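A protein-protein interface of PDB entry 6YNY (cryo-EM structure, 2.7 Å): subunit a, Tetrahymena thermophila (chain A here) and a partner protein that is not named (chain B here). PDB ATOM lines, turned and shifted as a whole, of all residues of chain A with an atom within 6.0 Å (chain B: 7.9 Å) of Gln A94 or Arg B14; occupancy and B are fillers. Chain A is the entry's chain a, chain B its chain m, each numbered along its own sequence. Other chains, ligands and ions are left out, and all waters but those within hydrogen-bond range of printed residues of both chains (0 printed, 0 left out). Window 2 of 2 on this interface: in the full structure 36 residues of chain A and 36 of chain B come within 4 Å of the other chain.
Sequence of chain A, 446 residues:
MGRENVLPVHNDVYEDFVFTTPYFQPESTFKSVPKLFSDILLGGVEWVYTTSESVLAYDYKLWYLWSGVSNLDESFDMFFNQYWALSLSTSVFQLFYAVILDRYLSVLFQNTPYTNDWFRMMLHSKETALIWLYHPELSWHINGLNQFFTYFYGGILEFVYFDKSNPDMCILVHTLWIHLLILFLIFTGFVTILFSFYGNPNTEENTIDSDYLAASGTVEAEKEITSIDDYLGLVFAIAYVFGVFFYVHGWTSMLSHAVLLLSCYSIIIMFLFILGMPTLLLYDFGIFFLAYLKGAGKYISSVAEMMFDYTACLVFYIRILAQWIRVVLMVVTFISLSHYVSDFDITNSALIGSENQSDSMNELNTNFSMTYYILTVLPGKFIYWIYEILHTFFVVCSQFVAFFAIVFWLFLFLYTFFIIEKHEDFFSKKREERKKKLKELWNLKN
The backbone carbonyl oxygen (O) of Ser A89 is in hydrogen-bond range of the side-chain amide nitrogen (NE2) of Gln A94, at 3.4 Å. The side-chain hydroxyl (OG) of Ser A87 sits at hydrogen-bond distance from the backbone carbonyl oxygen (O) of Trp A84. O of Ser A87 sits at hydrogen-bond distance from NE2 of Gln A94 (3.2 Å). The backbone carbonyl oxygen (O) of Phe B5 lies within hydrogen-bond range of the side-chain hydroxyl (OG1) of Thr B9. OG of Ser A91 lies close to N of Phe A93 (3.5 Å).
Among the printed residues, pairs that only touch across the chains: Leu A88 with Arg B14 (3.0 Å), Gln A94 with Arg B14 (3.2 Å), Val A92 with Ala B175 (3.4 Å), Ala A98 with Phe B5 (3.5 Å), Trp A84 with Phe B5 (3.6 Å), Ala A98 with Thr B9 (3.6 Å), Val A99 with Thr B6 (3.7 Å), Ala A98 with Thr B6 (3.8 Å), Val A99 with Leu B174 (3.8 Å), Phe A93 with Ala B175 (3.96 Å), Phe A96 with Leu B174 (3.98 Å) and Leu A95 with Leu B10 (3.98 Å).
Of the printed residues of chain B, Val A92 touches Ala B175 (3.4 Å). Gln A94 touches just one residue of chain B: Arg B14 (3.2 Å). Of the printed residues of chain A, Thr B9 touches Ala A98. Of the printed residues of chain A, Leu B10 touches Leu A95 (3.98 Å). Gly B12 touches none of the printed residues of chain A. The nearest residue of chain A that does not touch Arg B14 is Trp A84 (4.1 Å). The nearest printed residue of chain A that does not touch Thr B9 is Leu A95 (4.01 Å).
Printed residues of chain B that touch a printed residue of chain A: Phe B5, Thr B6, Thr B9, Leu B10, Arg B14, Leu B174 and Ala B175. Hydrophobic or aromatic side chains of chain B that line the printed part of chain A: Phe B5, Leu B10, Leu B174 and Ala B175.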
ATOM      1  N   TRP A  84      26.689 -35.731 -14.196  1.00  0.00           N
ATOM      2  CA  TRP A  84      25.476 -35.299 -14.877  1.00  0.00           C
ATOM      3  C   TRP A  84      24.238 -35.714 -14.099  1.00  0.00           C
ATOM      4  O   TRP A  84      23.364 -34.889 -13.817  1.00  0.00           O
ATOM      5  CB  TRP A  84      25.437 -35.873 -16.292  1.00  0.00           C
ATOM      6  CG  TRP A  84      24.119 -35.732 -16.956  1.00  0.00           C
ATOM      7  CD1 TRP A  84      23.544 -34.583 -17.395  1.00  0.00           C
ATOM      8  CD2 TRP A  84      23.203 -36.783 -17.264  1.00  0.00           C
ATOM      9  NE1 TRP A  84      22.324 -34.849 -17.956  1.00  0.00           N
ATOM     10  CE2 TRP A  84      22.091 -36.195 -17.887  1.00  0.00           C
ATOM     11  CE3 TRP A  84      23.215 -38.165 -17.072  1.00  0.00           C
ATOM     12  CZ2 TRP A  84      21.003 -36.940 -18.320  1.00  0.00           C
ATOM     13  CZ3 TRP A  84      22.138 -38.899 -17.499  1.00  0.00           C
ATOM     14  CH2 TRP A  84      21.047 -38.289 -18.117  1.00  0.00           C
ATOM     15  N   LEU A  86      24.178 -36.296 -11.095  1.00  0.00           N
ATOM     16  CA  LEU A  86      24.243 -35.549  -9.848  1.00  0.00           C
ATOM     17  C   LEU A  86      23.639 -34.159 -10.002  1.00  0.00           C
ATOM     18  O   LEU A  86      22.983 -33.656  -9.084  1.00  0.00           O
ATOM     19  CB  LEU A  86      25.693 -35.465  -9.394  1.00  0.00           C
ATOM     20  CG  LEU A  86      25.984 -34.797  -8.063  1.00  0.00           C
ATOM     21  CD1 LEU A  86      25.301 -35.536  -6.945  1.00  0.00           C
ATOM     22  CD2 LEU A  86      27.471 -34.770  -7.858  1.00  0.00           C
ATOM     23  N   SER A  87      23.852 -33.524 -11.153  1.00  0.00           N
ATOM     24  CA  SER A  87      23.295 -32.204 -11.408  1.00  0.00           C
ATOM     25  C   SER A  87      21.793 -32.229 -11.642  1.00  0.00           C
ATOM     26  O   SER A  87      21.165 -31.167 -11.613  1.00  0.00           O
ATOM     27  CB  SER A  87      23.984 -31.576 -12.617  1.00  0.00           C
ATOM     28  OG  SER A  87      23.737 -32.327 -13.790  1.00  0.00           O
ATOM     29  N   LEU A  88      21.204 -33.401 -11.874  1.00  0.00           N
ATOM     30  CA  LEU A  88      19.769 -33.475 -12.106  1.00  0.00           C
ATOM     31  C   LEU A  88      18.983 -33.313 -10.815  1.00  0.00           C
ATOM     32  O   LEU A  88      17.862 -32.794 -10.835  1.00  0.00           O
ATOM     33  CB  LEU A  88      19.414 -34.805 -12.767  1.00  0.00           C
ATOM     34  CG  LEU A  88      20.063 -35.090 -14.117  1.00  0.00           C
ATOM     35  CD1 LEU A  88      19.705 -36.476 -14.585  1.00  0.00           C
ATOM     36  CD2 LEU A  88      19.642 -34.073 -15.140  1.00  0.00           C
ATOM     37  N   SER A  89      19.551 -33.748  -9.697  1.00  0.00           N
ATOM     38  CA  SER A  89      18.890 -33.635  -8.410  1.00  0.00           C
ATOM     39  C   SER A  89      19.087 -32.242  -7.831  1.00  0.00           C
ATOM     40  O   SER A  89      20.122 -31.600  -8.032  1.00  0.00           O
ATOM     41  CB  SER A  89      19.425 -34.687  -7.443  1.00  0.00           C
ATOM     42  OG  SER A  89      20.834 -34.609  -7.333  1.00  0.00           O
ATOM     43  N   THR A  90      18.078 -31.777  -7.103  1.00  0.00           N
ATOM     44  CA  THR A  90      18.123 -30.439  -6.534  1.00  0.00           C
ATOM     45  C   THR A  90      19.153 -30.380  -5.416  1.00  0.00           C
ATOM     46  O   THR A  90      19.107 -31.170  -4.468  1.00  0.00           O
ATOM     47  CB  THR A  90      16.749 -30.034  -6.011  1.00  0.00           C
ATOM     48  OG1 THR A  90      15.795 -30.089  -7.077  1.00  0.00           O
ATOM     49  CG2 THR A  90      16.788 -28.628  -5.460  1.00  0.00           C
ATOM     50  N   SER A  91      20.085 -29.440  -5.534  1.00  0.00           N
ATOM     51  CA  SER A  91      21.143 -29.270  -4.554  1.00  0.00           C
ATOM     52  C   SER A  91      21.614 -27.825  -4.591  1.00  0.00           C
ATOM     53  O   SER A  91      21.289 -27.064  -5.505  1.00  0.00           O
ATOM     54  CB  SER A  91      22.309 -30.222  -4.815  1.00  0.00           C
ATOM     55  OG  SER A  91      23.354 -30.017  -3.883  1.00  0.00           O
ATOM     56  N   VAL A  92      22.391 -27.457  -3.574  1.00  0.00           N
ATOM     57  CA  VAL A  92      22.932 -26.107  -3.511  1.00  0.00           C
ATOM     58  C   VAL A  92      24.054 -25.923  -4.522  1.00  0.00           C
ATOM     59  O   VAL A  92      24.313 -24.802  -4.973  1.00  0.00           O
ATOM     60  CB  VAL A  92      23.398 -25.801  -2.077  1.00  0.00           C
ATOM     61  CG1 VAL A  92      24.634 -26.585  -1.744  1.00  0.00           C
ATOM     62  CG2 VAL A  92      23.642 -24.332  -1.902  1.00  0.00           C
ATOM     63  N   PHE A  93      24.730 -27.007  -4.904  1.00  0.00           N
ATOM     64  CA  PHE A  93      25.789 -26.958  -5.901  1.00  0.00           C
ATOM     65  C   PHE A  93      25.305 -27.362  -7.288  1.00  0.00           C
ATOM     66  O   PHE A  93      26.123 -27.697  -8.149  1.00  0.00           O
ATOM     67  CB  PHE A  93      26.949 -27.861  -5.484  1.00  0.00           C
ATOM     68  CG  PHE A  93      27.455 -27.604  -4.101  1.00  0.00           C
ATOM     69  CD1 PHE A  93      28.317 -26.559  -3.850  1.00  0.00           C
ATOM     70  CD2 PHE A  93      27.084 -28.423  -3.055  1.00  0.00           C
ATOM     71  CE1 PHE A  93      28.788 -26.327  -2.579  1.00  0.00           C
ATOM     72  CE2 PHE A  93      27.554 -28.196  -1.785  1.00  0.00           C
ATOM     73  CZ  PHE A  93      28.407 -27.147  -1.548  1.00  0.00           C
ATOM     74  N   GLN A  94      23.993 -27.332  -7.520  1.00  0.00           N
ATOM     75  CA  GLN A  94      23.455 -27.769  -8.804  1.00  0.00           C
ATOM     76  C   GLN A  94      24.075 -26.990  -9.956  1.00  0.00           C
ATOM     77  O   GLN A  94      24.308 -27.545 -11.036  1.00  0.00           O
ATOM     78  CB  GLN A  94      21.937 -27.614  -8.802  1.00  0.00           C
ATOM     79  CG  GLN A  94      21.231 -28.328  -9.922  1.00  0.00           C
ATOM     80  CD  GLN A  94      19.728 -28.234  -9.812  1.00  0.00           C
ATOM     81  OE1 GLN A  94      19.190 -27.244  -9.317  1.00  0.00           O
ATOM     82  NE2 GLN A  94      19.039 -29.270 -10.264  1.00  0.00           N
ATOM     83  N   LEU A  95      24.348 -25.702  -9.748  1.00  0.00           N
ATOM     84  CA  LEU A  95      24.961 -24.889 -10.789  1.00  0.00           C
ATOM     85  C   LEU A  95      26.465 -25.100 -10.870  1.00  0.00           C
ATOM     86  O   LEU A  95      27.046 -24.982 -11.954  1.00  0.00           O
ATOM     87  CB  LEU A  95      24.660 -23.416 -10.539  1.00  0.00           C
ATOM     88  CG  LEU A  95      25.305 -22.411 -11.486  1.00  0.00           C
ATOM     89  CD1 LEU A  95      24.872 -22.650 -12.906  1.00  0.00           C
ATOM     90  CD2 LEU A  95      24.954 -21.015 -11.058  1.00  0.00           C
ATOM     91  N   PHE A  96      27.109 -25.401  -9.744  1.00  0.00           N
ATOM     92  CA  PHE A  96      28.546 -25.638  -9.759  1.00  0.00           C
ATOM     93  C   PHE A  96      28.888 -26.905 -10.530  1.00  0.00           C
ATOM     94  O   PHE A  96      29.872 -26.938 -11.275  1.00  0.00           O
ATOM     95  CB  PHE A  96      29.069 -25.715  -8.328  1.00  0.00           C
ATOM     96  CG  PHE A  96      30.473 -26.208  -8.222  1.00  0.00           C
ATOM     97  CD1 PHE A  96      31.535 -25.368  -8.483  1.00  0.00           C
ATOM     98  CD2 PHE A  96      30.734 -27.509  -7.850  1.00  0.00           C
ATOM     99  CE1 PHE A  96      32.826 -25.818  -8.383  1.00  0.00           C
ATOM    100  CE2 PHE A  96      32.020 -27.965  -7.749  1.00  0.00           C
ATOM    101  CZ  PHE A  96      33.070 -27.117  -8.014  1.00  0.00           C
ATOM    102  N   TYR A  97      28.089 -27.959 -10.362  1.00  0.00           N
ATOM    103  CA  TYR A  97      28.332 -29.190 -11.102  1.00  0.00           C
ATOM    104  C   TYR A  97      28.185 -28.974 -12.599  1.00  0.00           C
ATOM    105  O   TYR A  97      28.857 -29.642 -13.392  1.00  0.00           O
ATOM    106  CB  TYR A  97      27.374 -30.281 -10.629  1.00  0.00           C
ATOM    107  CG  TYR A  97      27.488 -30.619  -9.165  1.00  0.00           C
ATOM    108  CD1 TYR A  97      28.703 -30.548  -8.509  1.00  0.00           C
ATOM    109  CD2 TYR A  97      26.378 -31.010  -8.438  1.00  0.00           C
ATOM    110  CE1 TYR A  97      28.810 -30.857  -7.176  1.00  0.00           C
ATOM    111  CE2 TYR A  97      26.476 -31.320  -7.105  1.00  0.00           C
ATOM    112  CZ  TYR A  97      27.694 -31.241  -6.478  1.00  0.00           C
ATOM    113  OH  TYR A  97      27.795 -31.550  -5.145  1.00  0.00           O
ATOM    114  N   ALA A  98      27.314 -28.052 -13.005  1.00  0.00           N
ATOM    115  CA  ALA A  98      27.153 -27.758 -14.422  1.00  0.00           C
ATOM    116  C   ALA A  98      28.404 -27.111 -14.995  1.00  0.00           C
ATOM    117  O   ALA A  98      28.794 -27.397 -16.131  1.00  0.00           O
ATOM    118  CB  ALA A  98      25.942 -26.855 -14.626  1.00  0.00           C
ATOM    119  N   VAL A  99      29.044 -26.234 -14.221  1.00  0.00           N
ATOM    120  CA  VAL A  99      30.263 -25.584 -14.681  1.00  0.00           C
ATOM    121  C   VAL A  99      31.405 -26.583 -14.765  1.00  0.00           C
ATOM    122  O   VAL A  99      32.258 -26.490 -15.654  1.00  0.00           O
ATOM    123  CB  VAL A  99      30.599 -24.406 -13.751  1.00  0.00           C
ATOM    124  CG1 VAL A  99      31.927 -23.785 -14.121  1.00  0.00           C
ATOM    125  CG2 VAL A  99      29.498 -23.372 -13.804  1.00  0.00           C
ATOM    126  N   TYR B   4      26.569 -25.612 -22.236  1.00  0.00           N
ATOM    127  CA  TYR B   4      25.233 -26.190 -22.317  1.00  0.00           C
ATOM    128  C   TYR B   4      24.638 -26.400 -20.931  1.00  0.00           C
ATOM    129  O   TYR B   4      23.580 -25.855 -20.604  1.00  0.00           O
ATOM    130  CB  TYR B   4      25.285 -27.508 -23.086  1.00  0.00           C
ATOM    131  CG  TYR B   4      24.027 -28.330 -22.963  1.00  0.00           C
ATOM    132  CD1 TYR B   4      22.954 -28.123 -23.811  1.00  0.00           C
ATOM    133  CD2 TYR B   4      23.912 -29.311 -21.995  1.00  0.00           C
ATOM    134  CE1 TYR B   4      21.808 -28.868 -23.696  1.00  0.00           C
ATOM    135  CE2 TYR B   4      22.772 -30.056 -21.874  1.00  0.00           C
ATOM    136  CZ  TYR B   4      21.723 -29.834 -22.725  1.00  0.00           C
ATOM    137  OH  TYR B   4      20.583 -30.583 -22.598  1.00  0.00           O
ATOM    138  N   PHE B   5      25.311 -27.197 -20.099  1.00  0.00           N
ATOM    139  CA  PHE B   5      24.762 -27.525 -18.790  1.00  0.00           C
ATOM    140  C   PHE B   5      24.575 -26.284 -17.933  1.00  0.00           C
ATOM    141  O   PHE B   5      23.633 -26.216 -17.137  1.00  0.00           O
ATOM    142  CB  PHE B   5      25.667 -28.527 -18.081  1.00  0.00           C
ATOM    143  CG  PHE B   5      25.770 -29.844 -18.779  1.00  0.00           C
ATOM    144  CD1 PHE B   5      26.946 -30.229 -19.387  1.00  0.00           C
ATOM    145  CD2 PHE B   5      24.686 -30.695 -18.837  1.00  0.00           C
ATOM    146  CE1 PHE B   5      27.038 -31.438 -20.029  1.00  0.00           C
ATOM    147  CE2 PHE B   5      24.775 -31.904 -19.479  1.00  0.00           C
ATOM    148  CZ  PHE B   5      25.950 -32.276 -20.076  1.00  0.00           C
ATOM    149  N   THR B   6      25.455 -25.296 -18.079  1.00  0.00           N
ATOM    150  CA  THR B   6      25.305 -24.060 -17.325  1.00  0.00           C
ATOM    151  C   THR B   6      24.050 -23.313 -17.751  1.00  0.00           C
ATOM    152  O   THR B   6      23.275 -22.847 -16.910  1.00  0.00           O
ATOM    153  CB  THR B   6      26.544 -23.186 -17.507  1.00  0.00           C
ATOM    154  OG1 THR B   6      27.700 -23.895 -17.048  1.00  0.00           O
ATOM    155  CG2 THR B   6      26.411 -21.904 -16.733  1.00  0.00           C
ATOM    156  N   ALA B   7      23.827 -23.198 -19.058  1.00  0.00           N
ATOM    157  CA  ALA B   7      22.655 -22.487 -19.549  1.00  0.00           C
ATOM    158  C   ALA B   7      21.374 -23.231 -19.199  1.00  0.00           C
ATOM    159  O   ALA B   7      20.399 -22.628 -18.739  1.00  0.00           O
ATOM    160  CB  ALA B   7      22.767 -22.285 -21.056  1.00  0.00           C
ATOM    161  N   ILE B   8      21.358 -24.548 -19.411  1.00  0.00           N
ATOM    162  CA  ILE B   8      20.178 -25.338 -19.082  1.00  0.00           C
ATOM    163  C   ILE B   8      19.840 -25.214 -17.606  1.00  0.00           C
ATOM    164  O   ILE B   8      18.669 -25.296 -17.219  1.00  0.00           O
ATOM    165  CB  ILE B   8      20.401 -26.806 -19.490  1.00  0.00           C
ATOM    166  CG1 ILE B   8      20.553 -26.926 -21.006  1.00  0.00           C
ATOM    167  CG2 ILE B   8      19.273 -27.678 -19.011  1.00  0.00           C
ATOM    168  CD1 ILE B   8      19.359 -26.466 -21.797  1.00  0.00           C
ATOM    169  N   THR B   9      20.847 -25.010 -16.760  1.00  0.00           N
ATOM    170  CA  THR B   9      20.606 -24.908 -15.327  1.00  0.00           C
ATOM    171  C   THR B   9      20.062 -23.537 -14.949  1.00  0.00           C
ATOM    172  O   THR B   9      19.192 -23.432 -14.079  1.00  0.00           O
ATOM    173  CB  THR B   9      21.893 -25.202 -14.566  1.00  0.00           C
ATOM    174  OG1 THR B   9      22.323 -26.537 -14.852  1.00  0.00           O
ATOM    175  CG2 THR B   9      21.675 -25.062 -13.087  1.00  0.00           C
ATOM    176  N   LEU B  10      20.560 -22.479 -15.588  1.00  0.00           N
ATOM    177  CA  LEU B  10      20.069 -21.141 -15.286  1.00  0.00           C
ATOM    178  C   LEU B  10      18.635 -20.956 -15.757  1.00  0.00           C
ATOM    179  O   LEU B  10      17.864 -20.231 -15.120  1.00  0.00           O
ATOM    180  CB  LEU B  10      20.972 -20.097 -15.934  1.00  0.00           C
ATOM    181  CG  LEU B  10      22.426 -20.096 -15.470  1.00  0.00           C
ATOM    182  CD1 LEU B  10      23.263 -19.223 -16.369  1.00  0.00           C
ATOM    183  CD2 LEU B  10      22.536 -19.630 -14.042  1.00  0.00           C
ATOM    184  N   LEU B  11      18.263 -21.594 -16.866  1.00  0.00           N
ATOM    185  CA  LEU B  11      16.892 -21.523 -17.346  1.00  0.00           C
ATOM    186  C   LEU B  11      15.922 -22.248 -16.427  1.00  0.00           C
ATOM    187  O   LEU B  11      14.714 -22.002 -16.506  1.00  0.00           O
ATOM    188  CB  LEU B  11      16.805 -22.114 -18.750  1.00  0.00           C
ATOM    189  CG  LEU B  11      17.639 -21.418 -19.821  1.00  0.00           C
ATOM    190  CD1 LEU B  11      17.603 -22.205 -21.110  1.00  0.00           C
ATOM    191  CD2 LEU B  11      17.151 -20.011 -20.044  1.00  0.00           C
ATOM    192  N   GLY B  12      16.418 -23.126 -15.564  1.00  0.00           N
ATOM    193  CA  GLY B  12      15.582 -23.856 -14.639  1.00  0.00           C
ATOM    194  C   GLY B  12      15.066 -25.182 -15.141  1.00  0.00           C
ATOM    195  O   GLY B  12      14.197 -25.773 -14.493  1.00  0.00           O
ATOM    196  N   LEU B  13      15.582 -25.681 -16.263  1.00  0.00           N
ATOM    197  CA  LEU B  13      15.104 -26.939 -16.816  1.00  0.00           C
ATOM    198  C   LEU B  13      15.426 -28.139 -15.941  1.00  0.00           C
ATOM    199  O   LEU B  13      14.988 -29.248 -16.262  1.00  0.00           O
ATOM    200  CB  LEU B  13      15.694 -27.147 -18.203  1.00  0.00           C
ATOM    201  CG  LEU B  13      15.041 -26.318 -19.305  1.00  0.00           C
ATOM    202  CD1 LEU B  13      15.802 -26.458 -20.599  1.00  0.00           C
ATOM    203  CD2 LEU B  13      13.600 -26.734 -19.489  1.00  0.00           C
ATOM    204  N   ARG B  14      16.177 -27.955 -14.860  1.00  0.00           N
ATOM    205  CA  ARG B  14      16.445 -29.039 -13.930  1.00  0.00           C
ATOM    206  C   ARG B  14      15.355 -29.202 -12.882  1.00  0.00           C
ATOM    207  O   ARG B  14      15.270 -30.267 -12.262  1.00  0.00           O
ATOM    208  CB  ARG B  14      17.779 -28.808 -13.220  1.00  0.00           C
ATOM    209  CG  ARG B  14      18.967 -28.705 -14.143  1.00  0.00           C
ATOM    210  CD  ARG B  14      19.082 -29.928 -15.015  1.00  0.00           C
ATOM    211  NE  ARG B  14      20.360 -29.998 -15.706  1.00  0.00           N
ATOM    212  CZ  ARG B  14      20.623 -30.865 -16.673  1.00  0.00           C
ATOM    213  NH1 ARG B  14      19.697 -31.720 -17.063  1.00  0.00           N
ATOM    214  NH2 ARG B  14      21.810 -30.873 -17.256  1.00  0.00           N
ATOM    215  N   ASP B  15      14.524 -28.183 -12.681  1.00  0.00           N
ATOM    216  CA  ASP B  15      13.498 -28.207 -11.649  1.00  0.00           C
ATOM    217  C   ASP B  15      12.121 -27.784 -12.127  1.00  0.00           C
ATOM    218  O   ASP B  15      11.137 -28.095 -11.445  1.00  0.00           O
ATOM    219  CB  ASP B  15      13.904 -27.299 -10.479  1.00  0.00           C
ATOM    220  CG  ASP B  15      14.190 -25.877 -10.921  1.00  0.00           C
ATOM    221  OD1 ASP B  15      13.241 -25.176 -11.327  1.00  0.00           O
ATOM    222  OD2 ASP B  15      15.367 -25.462 -10.864  1.00  0.00           O
ATOM    223  N   GLN B  16      12.006 -27.096 -13.258  1.00  0.00           N
ATOM    224  CA  GLN B  16      10.725 -26.608 -13.739  1.00  0.00           C
ATOM    225  C   GLN B  16      10.696 -26.753 -15.255  1.00  0.00           C
ATOM    226  O   GLN B  16      11.578 -27.369 -15.859  1.00  0.00           O
ATOM    227  CB  GLN B  16      10.499 -25.160 -13.289  1.00  0.00           C
ATOM    228  CG  GLN B  16      11.406 -24.153 -13.954  1.00  0.00           C
ATOM    229  CD  GLN B  16      11.409 -22.818 -13.248  1.00  0.00           C
ATOM    230  OE1 GLN B  16      10.993 -21.805 -13.806  1.00  0.00           O
ATOM    231  NE2 GLN B  16      11.890 -22.809 -12.011  1.00  0.00           N
ATOM    232  N   ASN B  17       9.664 -26.184 -15.872  1.00  0.00           N
ATOM    233  CA  ASN B  17       9.477 -26.250 -17.310  1.00  0.00           C
ATOM    234  C   ASN B  17       9.317 -24.846 -17.869  1.00  0.00           C
ATOM    235  O   ASN B  17       8.806 -23.946 -17.200  1.00  0.00           O
ATOM    236  CB  ASN B  17       8.256 -27.096 -17.674  1.00  0.00           C
ATOM    237  CG  ASN B  17       8.378 -28.526 -17.203  1.00  0.00           C
ATOM    238  OD1 ASN B  17       9.450 -29.125 -17.266  1.00  0.00           O
ATOM    239  ND2 ASN B  17       7.278 -29.079 -16.721  1.00  0.00           N
ATOM    240  N   LEU B 174      29.392 -19.960  -6.594  1.00  0.00           N
ATOM    241  CA  LEU B 174      28.319 -20.448  -7.451  1.00  0.00           C
ATOM    242  C   LEU B 174      27.186 -21.066  -6.647  1.00  0.00           C
ATOM    243  O   LEU B 174      26.037 -21.066  -7.099  1.00  0.00           O
ATOM    244  CB  LEU B 174      28.863 -21.467  -8.446  1.00  0.00           C
ATOM    245  CG  LEU B 174      29.845 -20.932  -9.481  1.00  0.00           C
ATOM    246  CD1 LEU B 174      30.351 -22.055 -10.346  1.00  0.00           C
ATOM    247  CD2 LEU B 174      29.193 -19.866 -10.326  1.00  0.00           C
ATOM    248  N   ALA B 175      27.485 -21.599  -5.464  1.00  0.00           N
ATOM    249  CA  ALA B 175      26.427 -22.104  -4.603  1.00  0.00           C
ATOM    250  C   ALA B 175      25.516 -20.983  -4.128  1.00  0.00           C
ATOM    251  O   ALA B 175      24.323 -21.206  -3.903  1.00  0.00           O
ATOM    252  CB  ALA B 175      27.033 -22.838  -3.412  1.00  0.00           C
